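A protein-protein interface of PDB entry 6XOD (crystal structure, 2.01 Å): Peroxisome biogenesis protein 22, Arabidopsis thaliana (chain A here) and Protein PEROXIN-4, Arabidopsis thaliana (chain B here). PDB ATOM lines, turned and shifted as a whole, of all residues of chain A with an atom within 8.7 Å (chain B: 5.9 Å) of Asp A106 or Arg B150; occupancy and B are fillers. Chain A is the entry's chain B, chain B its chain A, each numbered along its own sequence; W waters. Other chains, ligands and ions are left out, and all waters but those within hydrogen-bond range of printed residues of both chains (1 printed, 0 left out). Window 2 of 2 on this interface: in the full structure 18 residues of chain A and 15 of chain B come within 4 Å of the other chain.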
ATOM      1  N   LEU A  73     -25.236   4.382 -17.474  1.00  0.00           N
ATOM      2  CA  LEU A  73     -24.883   5.719 -17.018  1.00  0.00           C
ATOM      3  C   LEU A  73     -23.584   6.184 -17.658  1.00  0.00           C
ATOM      4  O   LEU A  73     -22.631   5.410 -17.794  1.00  0.00           O
ATOM      5  CB  LEU A  73     -24.743   5.763 -15.488  1.00  0.00           C
ATOM      6  CG  LEU A  73     -24.254   7.085 -14.891  1.00  0.00           C
ATOM      7  CD1 LEU A  73     -25.227   8.212 -15.199  1.00  0.00           C
ATOM      8  CD2 LEU A  73     -24.041   6.947 -13.390  1.00  0.00           C
ATOM      9  N   TYR A  74     -23.553   7.464 -18.030  1.00  0.00           N
ATOM     10  CA  TYR A  74     -22.367   8.110 -18.575  1.00  0.00           C
ATOM     11  C   TYR A  74     -22.128   9.403 -17.813  1.00  0.00           C
ATOM     12  O   TYR A  74     -22.963  10.313 -17.854  1.00  0.00           O
ATOM     13  CB  TYR A  74     -22.527   8.395 -20.071  1.00  0.00           C
ATOM     14  CG  TYR A  74     -22.783   7.154 -20.881  1.00  0.00           C
ATOM     15  CD1 TYR A  74     -24.059   6.612 -20.969  1.00  0.00           C
ATOM     16  CD2 TYR A  74     -21.752   6.516 -21.551  1.00  0.00           C
ATOM     17  CE1 TYR A  74     -24.295   5.475 -21.698  1.00  0.00           C
ATOM     18  CE2 TYR A  74     -21.981   5.376 -22.285  1.00  0.00           C
ATOM     19  CZ  TYR A  74     -23.255   4.860 -22.356  1.00  0.00           C
ATOM     20  OH  TYR A  74     -23.494   3.722 -23.085  1.00  0.00           O
ATOM     21  N   LEU A  75     -21.001   9.479 -17.115  1.00  0.00           N
ATOM     22  CA  LEU A  75     -20.596  10.696 -16.430  1.00  0.00           C
ATOM     23  C   LEU A  75     -19.668  11.505 -17.328  1.00  0.00           C
ATOM     24  O   LEU A  75     -18.890  10.954 -18.108  1.00  0.00           O
ATOM     25  CB  LEU A  75     -19.901  10.363 -15.109  1.00  0.00           C
ATOM     26  CG  LEU A  75     -20.729   9.530 -14.126  1.00  0.00           C
ATOM     27  CD1 LEU A  75     -19.971   9.305 -12.828  1.00  0.00           C
ATOM     28  CD2 LEU A  75     -22.071  10.196 -13.846  1.00  0.00           C
ATOM     29  N   GLU A  85      -8.366  14.714 -14.931  1.00  0.00           N
ATOM     30  CA  GLU A  85      -9.063  13.476 -15.267  1.00  0.00           C
ATOM     31  C   GLU A  85      -8.692  12.365 -14.295  1.00  0.00           C
ATOM     32  O   GLU A  85      -9.564  11.664 -13.769  1.00  0.00           O
ATOM     33  CB  GLU A  85      -8.733  13.062 -16.702  1.00  0.00           C
ATOM     34  CG  GLU A  85      -9.168  14.066 -17.760  1.00  0.00           C
ATOM     35  CD  GLU A  85      -9.000  13.535 -19.170  1.00  0.00           C
ATOM     36  OE1 GLU A  85      -8.590  12.364 -19.320  1.00  0.00           O
ATOM     37  OE2 GLU A  85      -9.276  14.288 -20.126  1.00  0.00           O
ATOM     38  N   LEU A  89     -11.150  10.245 -11.725  1.00  0.00           N
ATOM     39  CA  LEU A  89     -11.327   8.798 -11.765  1.00  0.00           C
ATOM     40  C   LEU A  89     -10.965   8.159 -10.430  1.00  0.00           C
ATOM     41  O   LEU A  89     -11.625   7.211  -9.988  1.00  0.00           O
ATOM     42  CB  LEU A  89     -10.488   8.196 -12.891  1.00  0.00           C
ATOM     43  CG  LEU A  89     -10.917   8.563 -14.314  1.00  0.00           C
ATOM     44  CD1 LEU A  89      -9.972   7.945 -15.333  1.00  0.00           C
ATOM     45  CD2 LEU A  89     -12.354   8.126 -14.579  1.00  0.00           C
ATOM     46  N   LEU A  92     -13.922   8.808  -8.001  1.00  0.00           N
ATOM     47  CA  LEU A  92     -15.040   7.899  -8.232  1.00  0.00           C
ATOM     48  C   LEU A  92     -14.729   6.511  -7.691  1.00  0.00           C
ATOM     49  O   LEU A  92     -15.605   5.837  -7.137  1.00  0.00           O
ATOM     50  CB  LEU A  92     -15.362   7.823  -9.725  1.00  0.00           C
ATOM     51  CG  LEU A  92     -15.711   9.139 -10.423  1.00  0.00           C
ATOM     52  CD1 LEU A  92     -16.083   8.896 -11.878  1.00  0.00           C
ATOM     53  CD2 LEU A  92     -16.831   9.855  -9.696  1.00  0.00           C
ATOM     54  N   PHE A  98     -17.719   2.604  -9.185  1.00  0.00           N
ATOM     55  CA  PHE A  98     -17.620   1.574 -10.212  1.00  0.00           C
ATOM     56  C   PHE A  98     -17.899   0.216  -9.580  1.00  0.00           C
ATOM     57  O   PHE A  98     -17.246  -0.165  -8.602  1.00  0.00           O
ATOM     58  CB  PHE A  98     -16.239   1.584 -10.866  1.00  0.00           C
ATOM     59  CG  PHE A  98     -15.838   2.921 -11.414  1.00  0.00           C
ATOM     60  CD1 PHE A  98     -16.561   3.509 -12.438  1.00  0.00           C
ATOM     61  CD2 PHE A  98     -14.736   3.591 -10.908  1.00  0.00           C
ATOM     62  CE1 PHE A  98     -16.197   4.742 -12.944  1.00  0.00           C
ATOM     63  CE2 PHE A  98     -14.364   4.822 -11.412  1.00  0.00           C
ATOM     64  CZ  PHE A  98     -15.095   5.398 -12.433  1.00  0.00           C
ATOM     65  N   LEU A 103     -21.544   1.078 -13.168  1.00  0.00           N
ATOM     66  CA  LEU A 103     -20.739   2.003 -13.951  1.00  0.00           C
ATOM     67  C   LEU A 103     -19.324   1.472 -14.135  1.00  0.00           C
ATOM     68  O   LEU A 103     -18.740   0.886 -13.220  1.00  0.00           O
ATOM     69  CB  LEU A 103     -20.695   3.371 -13.270  1.00  0.00           C
ATOM     70  CG  LEU A 103     -19.901   4.460 -13.993  1.00  0.00           C
ATOM     71  CD1 LEU A 103     -20.532   4.791 -15.333  1.00  0.00           C
ATOM     72  CD2 LEU A 103     -19.799   5.701 -13.126  1.00  0.00           C
ATOM     73  N   VAL A 104     -18.775   1.692 -15.328  1.00  0.00           N
ATOM     74  CA  VAL A 104     -17.403   1.329 -15.654  1.00  0.00           C
ATOM     75  C   VAL A 104     -16.619   2.607 -15.920  1.00  0.00           C
ATOM     76  O   VAL A 104     -17.174   3.644 -16.291  1.00  0.00           O
ATOM     77  CB  VAL A 104     -17.323   0.378 -16.867  1.00  0.00           C
ATOM     78  CG1 VAL A 104     -17.812  -1.005 -16.487  1.00  0.00           C
ATOM     79  CG2 VAL A 104     -18.130   0.931 -18.041  1.00  0.00           C
ATOM     80  N   LYS A 105     -15.297   2.519 -15.731  1.00  0.00           N
ATOM     81  CA  LYS A 105     -14.446   3.694 -15.887  1.00  0.00           C
ATOM     82  C   LYS A 105     -14.446   4.207 -17.320  1.00  0.00           C
ATOM     83  O   LYS A 105     -14.242   5.406 -17.549  1.00  0.00           O
ATOM     84  CB  LYS A 105     -13.022   3.359 -15.445  1.00  0.00           C
ATOM     85  CG  LYS A 105     -12.930   2.942 -13.986  1.00  0.00           C
ATOM     86  CD  LYS A 105     -11.710   2.082 -13.705  1.00  0.00           C
ATOM     87  CE  LYS A 105     -11.913   1.259 -12.443  1.00  0.00           C
ATOM     88  NZ  LYS A 105     -12.777   0.069 -12.671  1.00  0.00           N
ATOM     89  N   ASP A 106     -14.669   3.326 -18.294  1.00  0.00           N
ATOM     90  CA  ASP A 106     -14.680   3.744 -19.690  1.00  0.00           C
ATOM     91  C   ASP A 106     -15.826   4.694 -20.008  1.00  0.00           C
ATOM     92  O   ASP A 106     -15.742   5.438 -20.991  1.00  0.00           O
ATOM     93  CB  ASP A 106     -14.761   2.521 -20.602  1.00  0.00           C
ATOM     94  CG  ASP A 106     -13.483   1.703 -20.594  1.00  0.00           C
ATOM     95  OD1 ASP A 106     -12.406   2.285 -20.351  1.00  0.00           O
ATOM     96  OD2 ASP A 106     -13.553   0.483 -20.832  1.00  0.00           O
ATOM     97  N   LYS A 107     -16.891   4.690 -19.206  1.00  0.00           N
ATOM     98  CA  LYS A 107     -18.054   5.535 -19.449  1.00  0.00           C
ATOM     99  C   LYS A 107     -18.020   6.813 -18.619  1.00  0.00           C
ATOM    100  O   LYS A 107     -19.068   7.329 -18.216  1.00  0.00           O
ATOM    101  CB  LYS A 107     -19.337   4.742 -19.197  1.00  0.00           C
ATOM    102  CG  LYS A 107     -19.519   3.627 -20.217  1.00  0.00           C
ATOM    103  CD  LYS A 107     -20.804   2.840 -20.042  1.00  0.00           C
ATOM    104  CE  LYS A 107     -21.031   1.931 -21.247  1.00  0.00           C
ATOM    105  NZ  LYS A 107     -22.288   1.137 -21.151  1.00  0.00           N
ATOM    106  N   VAL A 108     -16.823   7.332 -18.359  1.00  0.00           N
ATOM    107  CA  VAL A 108     -16.627   8.652 -17.774  1.00  0.00           C
ATOM    108  C   VAL A 108     -15.917   9.498 -18.821  1.00  0.00           C
ATOM    109  O   VAL A 108     -14.778   9.197 -19.202  1.00  0.00           O
ATOM    110  CB  VAL A 108     -15.817   8.594 -16.470  1.00  0.00           C
ATOM    111  CG1 VAL A 108     -15.695   9.984 -15.863  1.00  0.00           C
ATOM    112  CG2 VAL A 108     -16.463   7.632 -15.489  1.00  0.00           C
ATOM    113  N   LEU A 109     -16.588  10.548 -19.286  1.00  0.00           N
ATOM    114  CA  LEU A 109     -16.126  11.355 -20.403  1.00  0.00           C
ATOM    115  C   LEU A 109     -15.617  12.704 -19.916  1.00  0.00           C
ATOM    116  O   LEU A 109     -15.993  13.192 -18.847  1.00  0.00           O
ATOM    117  CB  LEU A 109     -17.251  11.553 -21.424  1.00  0.00           C
ATOM    118  CG  LEU A 109     -17.733  10.280 -22.122  1.00  0.00           C
ATOM    119  CD1 LEU A 109     -19.198  10.410 -22.533  1.00  0.00           C
ATOM    120  CD2 LEU A 109     -16.865   9.970 -23.334  1.00  0.00           C
ATOM    121  N   PHE A 110     -14.750  13.309 -20.724  1.00  0.00           N
ATOM    122  CA  PHE A 110     -14.120  14.575 -20.386  1.00  0.00           C
ATOM    123  C   PHE A 110     -14.065  15.458 -21.620  1.00  0.00           C
ATOM    124  O   PHE A 110     -13.868  14.969 -22.735  1.00  0.00           O
ATOM    125  CB  PHE A 110     -12.707  14.363 -19.833  1.00  0.00           C
ATOM    126  CG  PHE A 110     -12.670  13.584 -18.552  1.00  0.00           C
ATOM    127  CD1 PHE A 110     -13.003  14.188 -17.352  1.00  0.00           C
ATOM    128  CD2 PHE A 110     -12.303  12.249 -18.546  1.00  0.00           C
ATOM    129  CE1 PHE A 110     -12.972  13.477 -16.169  1.00  0.00           C
ATOM    130  CE2 PHE A 110     -12.269  11.531 -17.366  1.00  0.00           C
ATOM    131  CZ  PHE A 110     -12.605  12.147 -16.175  1.00  0.00           C
ATOM    132  N   ALA B 145     -14.409   9.541 -28.729  1.00  0.00           N
ATOM    133  CA  ALA B 145     -13.905   8.612 -29.734  1.00  0.00           C
ATOM    134  C   ALA B 145     -13.160   7.457 -29.079  1.00  0.00           C
ATOM    135  O   ALA B 145     -13.252   6.311 -29.532  1.00  0.00           O
ATOM    136  CB  ALA B 145     -13.000   9.341 -30.727  1.00  0.00           C
ATOM    137  N   GLN B 146     -12.422   7.740 -28.004  1.00  0.00           N
ATOM    138  CA  GLN B 146     -11.715   6.682 -27.292  1.00  0.00           C
ATOM    139  C   GLN B 146     -12.686   5.749 -26.576  1.00  0.00           C
ATOM    140  O   GLN B 146     -12.492   4.528 -26.573  1.00  0.00           O
ATOM    141  CB  GLN B 146     -10.724   7.293 -26.301  1.00  0.00           C
ATOM    142  CG  GLN B 146      -9.949   6.277 -25.478  1.00  0.00           C
ATOM    143  CD  GLN B 146      -9.006   6.930 -24.490  1.00  0.00           C
ATOM    144  OE1 GLN B 146      -9.439   7.554 -23.521  1.00  0.00           O
ATOM    145  NE2 GLN B 146      -7.710   6.796 -24.736  1.00  0.00           N
ATOM    146  N   MET B 147     -13.731   6.300 -25.953  1.00  0.00           N
ATOM    147  CA  MET B 147     -14.720   5.454 -25.294  1.00  0.00           C
ATOM    148  C   MET B 147     -15.317   4.455 -26.278  1.00  0.00           C
ATOM    149  O   MET B 147     -15.368   3.249 -26.008  1.00  0.00           O
ATOM    150  CB  MET B 147     -15.821   6.315 -24.674  1.00  0.00           C
ATOM    151  CG  MET B 147     -16.908   5.505 -23.977  1.00  0.00           C
ATOM    152  SD  MET B 147     -18.302   6.495 -23.392  1.00  0.00           S
ATOM    153  CE  MET B 147     -19.117   6.889 -24.937  1.00  0.00           C
ATOM    154  N   TYR B 148     -15.773   4.940 -27.432  1.00  0.00           N
ATOM    155  CA  TYR B 148     -16.355   4.042 -28.419  1.00  0.00           C
ATOM    156  C   TYR B 148     -15.325   3.054 -28.950  1.00  0.00           C
ATOM    157  O   TYR B 148     -15.672   1.912 -29.275  1.00  0.00           O
ATOM    158  CB  TYR B 148     -16.974   4.847 -29.559  1.00  0.00           C
ATOM    159  CG  TYR B 148     -18.360   5.360 -29.233  1.00  0.00           C
ATOM    160  CD1 TYR B 148     -19.419   4.480 -29.073  1.00  0.00           C
ATOM    161  CD2 TYR B 148     -18.607   6.719 -29.082  1.00  0.00           C
ATOM    162  CE1 TYR B 148     -20.689   4.935 -28.776  1.00  0.00           C
ATOM    163  CE2 TYR B 148     -19.875   7.184 -28.785  1.00  0.00           C
ATOM    164  CZ  TYR B 148     -20.911   6.284 -28.632  1.00  0.00           C
ATOM    165  OH  TYR B 148     -22.179   6.729 -28.338  1.00  0.00           O
ATOM    166  N   THR B 149     -14.059   3.463 -29.040  1.00  0.00           N
ATOM    167  CA  THR B 149     -13.014   2.517 -29.418  1.00  0.00           C
ATOM    168  C   THR B 149     -12.884   1.412 -28.376  1.00  0.00           C
ATOM    169  O   THR B 149     -12.740   0.234 -28.724  1.00  0.00           O
ATOM    170  CB  THR B 149     -11.679   3.241 -29.598  1.00  0.00           C
ATOM    171  OG1 THR B 149     -11.772   4.175 -30.681  1.00  0.00           O
ATOM    172  CG2 THR B 149     -10.566   2.241 -29.894  1.00  0.00           C
ATOM    173  N   ARG B 150     -12.941   1.773 -27.091  1.00  0.00           N
ATOM    174  CA  ARG B 150     -12.809   0.778 -26.034  1.00  0.00           C
ATOM    175  C   ARG B 150     -14.047  -0.103 -25.922  1.00  0.00           C
ATOM    176  O   ARG B 150     -13.941  -1.269 -25.524  1.00  0.00           O
ATOM    177  CB  ARG B 150     -12.547   1.466 -24.693  1.00  0.00           C
ATOM    178  CG  ARG B 150     -11.222   2.196 -24.605  1.00  0.00           C
ATOM    179  CD  ARG B 150     -11.141   3.003 -23.319  1.00  0.00           C
ATOM    180  NE  ARG B 150      -9.834   3.629 -23.134  1.00  0.00           N
ATOM    181  CZ  ARG B 150      -9.560   4.531 -22.197  1.00  0.00           C
ATOM    182  NH1 ARG B 150     -10.507   4.928 -21.354  1.00  0.00           N
ATOM    183  NH2 ARG B 150      -8.341   5.041 -22.105  1.00  0.00           N
ATOM    184  N   LEU B 151     -15.222   0.430 -26.253  1.00  0.00           N
ATOM    185  CA  LEU B 151     -16.461  -0.314 -26.072  1.00  0.00           C
ATOM    186  C   LEU B 151     -16.861  -1.122 -27.297  1.00  0.00           C
ATOM    187  O   LEU B 151     -17.565  -2.129 -27.159  1.00  0.00           O
ATOM    188  CB  LEU B 151     -17.611   0.637 -25.728  1.00  0.00           C
ATOM    189  CG  LEU B 151     -17.498   1.463 -24.447  1.00  0.00           C
ATOM    190  CD1 LEU B 151     -18.671   2.428 -24.358  1.00  0.00           C
ATOM    191  CD2 LEU B 151     -17.444   0.579 -23.215  1.00  0.00           C
ATOM    192  N   ALA B 152     -16.435  -0.707 -28.490  1.00  0.00           N
ATOM    193  CA  ALA B 152     -16.925  -1.295 -29.725  1.00  0.00           C
ATOM    194  C   ALA B 152     -15.840  -1.848 -30.636  1.00  0.00           C
ATOM    195  O   ALA B 152     -16.169  -2.599 -31.562  1.00  0.00           O
ATOM    196  CB  ALA B 152     -17.739  -0.258 -30.516  1.00  0.00           C
ATOM    197  N   ALA B 153     -14.568  -1.508 -30.415  1.00  0.00           N
ATOM    198  CA  ALA B 153     -13.508  -1.861 -31.353  1.00  0.00           C
ATOM    199  C   ALA B 153     -12.342  -2.571 -30.671  1.00  0.00           C
ATOM    200  O   ALA B 153     -11.214  -2.538 -31.173  1.00  0.00           O
ATOM    201  CB  ALA B 153     -13.007  -0.618 -32.089  1.00  0.00           C
ATOM    202  N   MET B 154     -12.592  -3.237 -29.545  1.00  0.00           N
ATOM    203  CA  MET B 154     -11.566  -3.999 -28.834  1.00  0.00           C
ATOM    204  C   MET B 154     -12.113  -5.375 -28.481  1.00  0.00           C
ATOM    205  O   MET B 154     -12.491  -5.629 -27.329  1.00  0.00           O
ATOM    206  CB  MET B 154     -11.104  -3.264 -27.573  1.00  0.00           C
ATOM    207  CG  MET B 154     -10.291  -2.009 -27.844  1.00  0.00           C
ATOM    208  SD  MET B 154      -9.554  -1.343 -26.339  1.00  0.00           S
ATOM    209  CE  MET B 154      -8.833   0.180 -26.943  1.00  0.00           C
HETATM  210  O   HOH W   1     -13.370   5.545 -22.271  1.00  0.00           O
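OD1 of Asp A106 is in salt-bridge range of NH1 of Arg B150 (3.4 Å). O of Asp A106 lies close to SD of Met B147, at 3.7 Å.
Of chain B, only Met B147 (3.2 Å) and Arg B150 (3.3 Å) come within 4 Å of Asp A106. Printed residues of chain A within 4 Å of Arg B150: Asp A106 (3.3 Å). Of the printed residues of chain A, Met B147 touches Tyr A74, Asp A106 and Leu A109. Printed residues of chain B within 4 Å of Leu A109: Met B147 (3.8 Å). Of the printed residues of chain A, Leu B151 touches Lys A107. Printed residues of chain B within 4 Å of Lys A107: Leu B151 (3.9 Å). Ala B145 touches none of the printed residues of chain A. The nearest printed residue of chain A that does not touch Met B147 is Lys A107 (4.1 Å).
Printed residues of chain A that touch a printed residue of chain B: Tyr A74, Asp A106, Lys A107 and Leu A109. Hydrophobic or aromatic side chains of chain B that line the printed part of chain A: Met B147 and Leu B151. Among the printed residues, 5 pairs touch across the chains.
The side-chain amide oxygen (OE1) of Gln B146 is in hydrogen-bond range of the guanidinium group (NH2) of Arg B150, 3.1 Å away. OH of Tyr A74 is in hydrogen-bond range of NZ of Lys A107 (3.4 Å). N of Leu A75 lies within hydrogen-bond range of O of Lys A107 (3.1 Å). The backbone NH (N) of Leu A109 sits at hydrogen-bond distance from the backbone carbonyl oxygen (O) of Leu A75 (2.6 Å).
Among the printed residues, pairs that only touch across the chains: Leu A109 with Met B147 (3.8 Å), Tyr A74 with Met B147 (3.9 Å) and Lys A107 with Leu B151 (3.9 Å).
Water W1 lies within hydrogen-bond range of the backbone carbonyl oxygen (O) of Asp A106 and the guanidinium group (NH1) of Arg B150.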
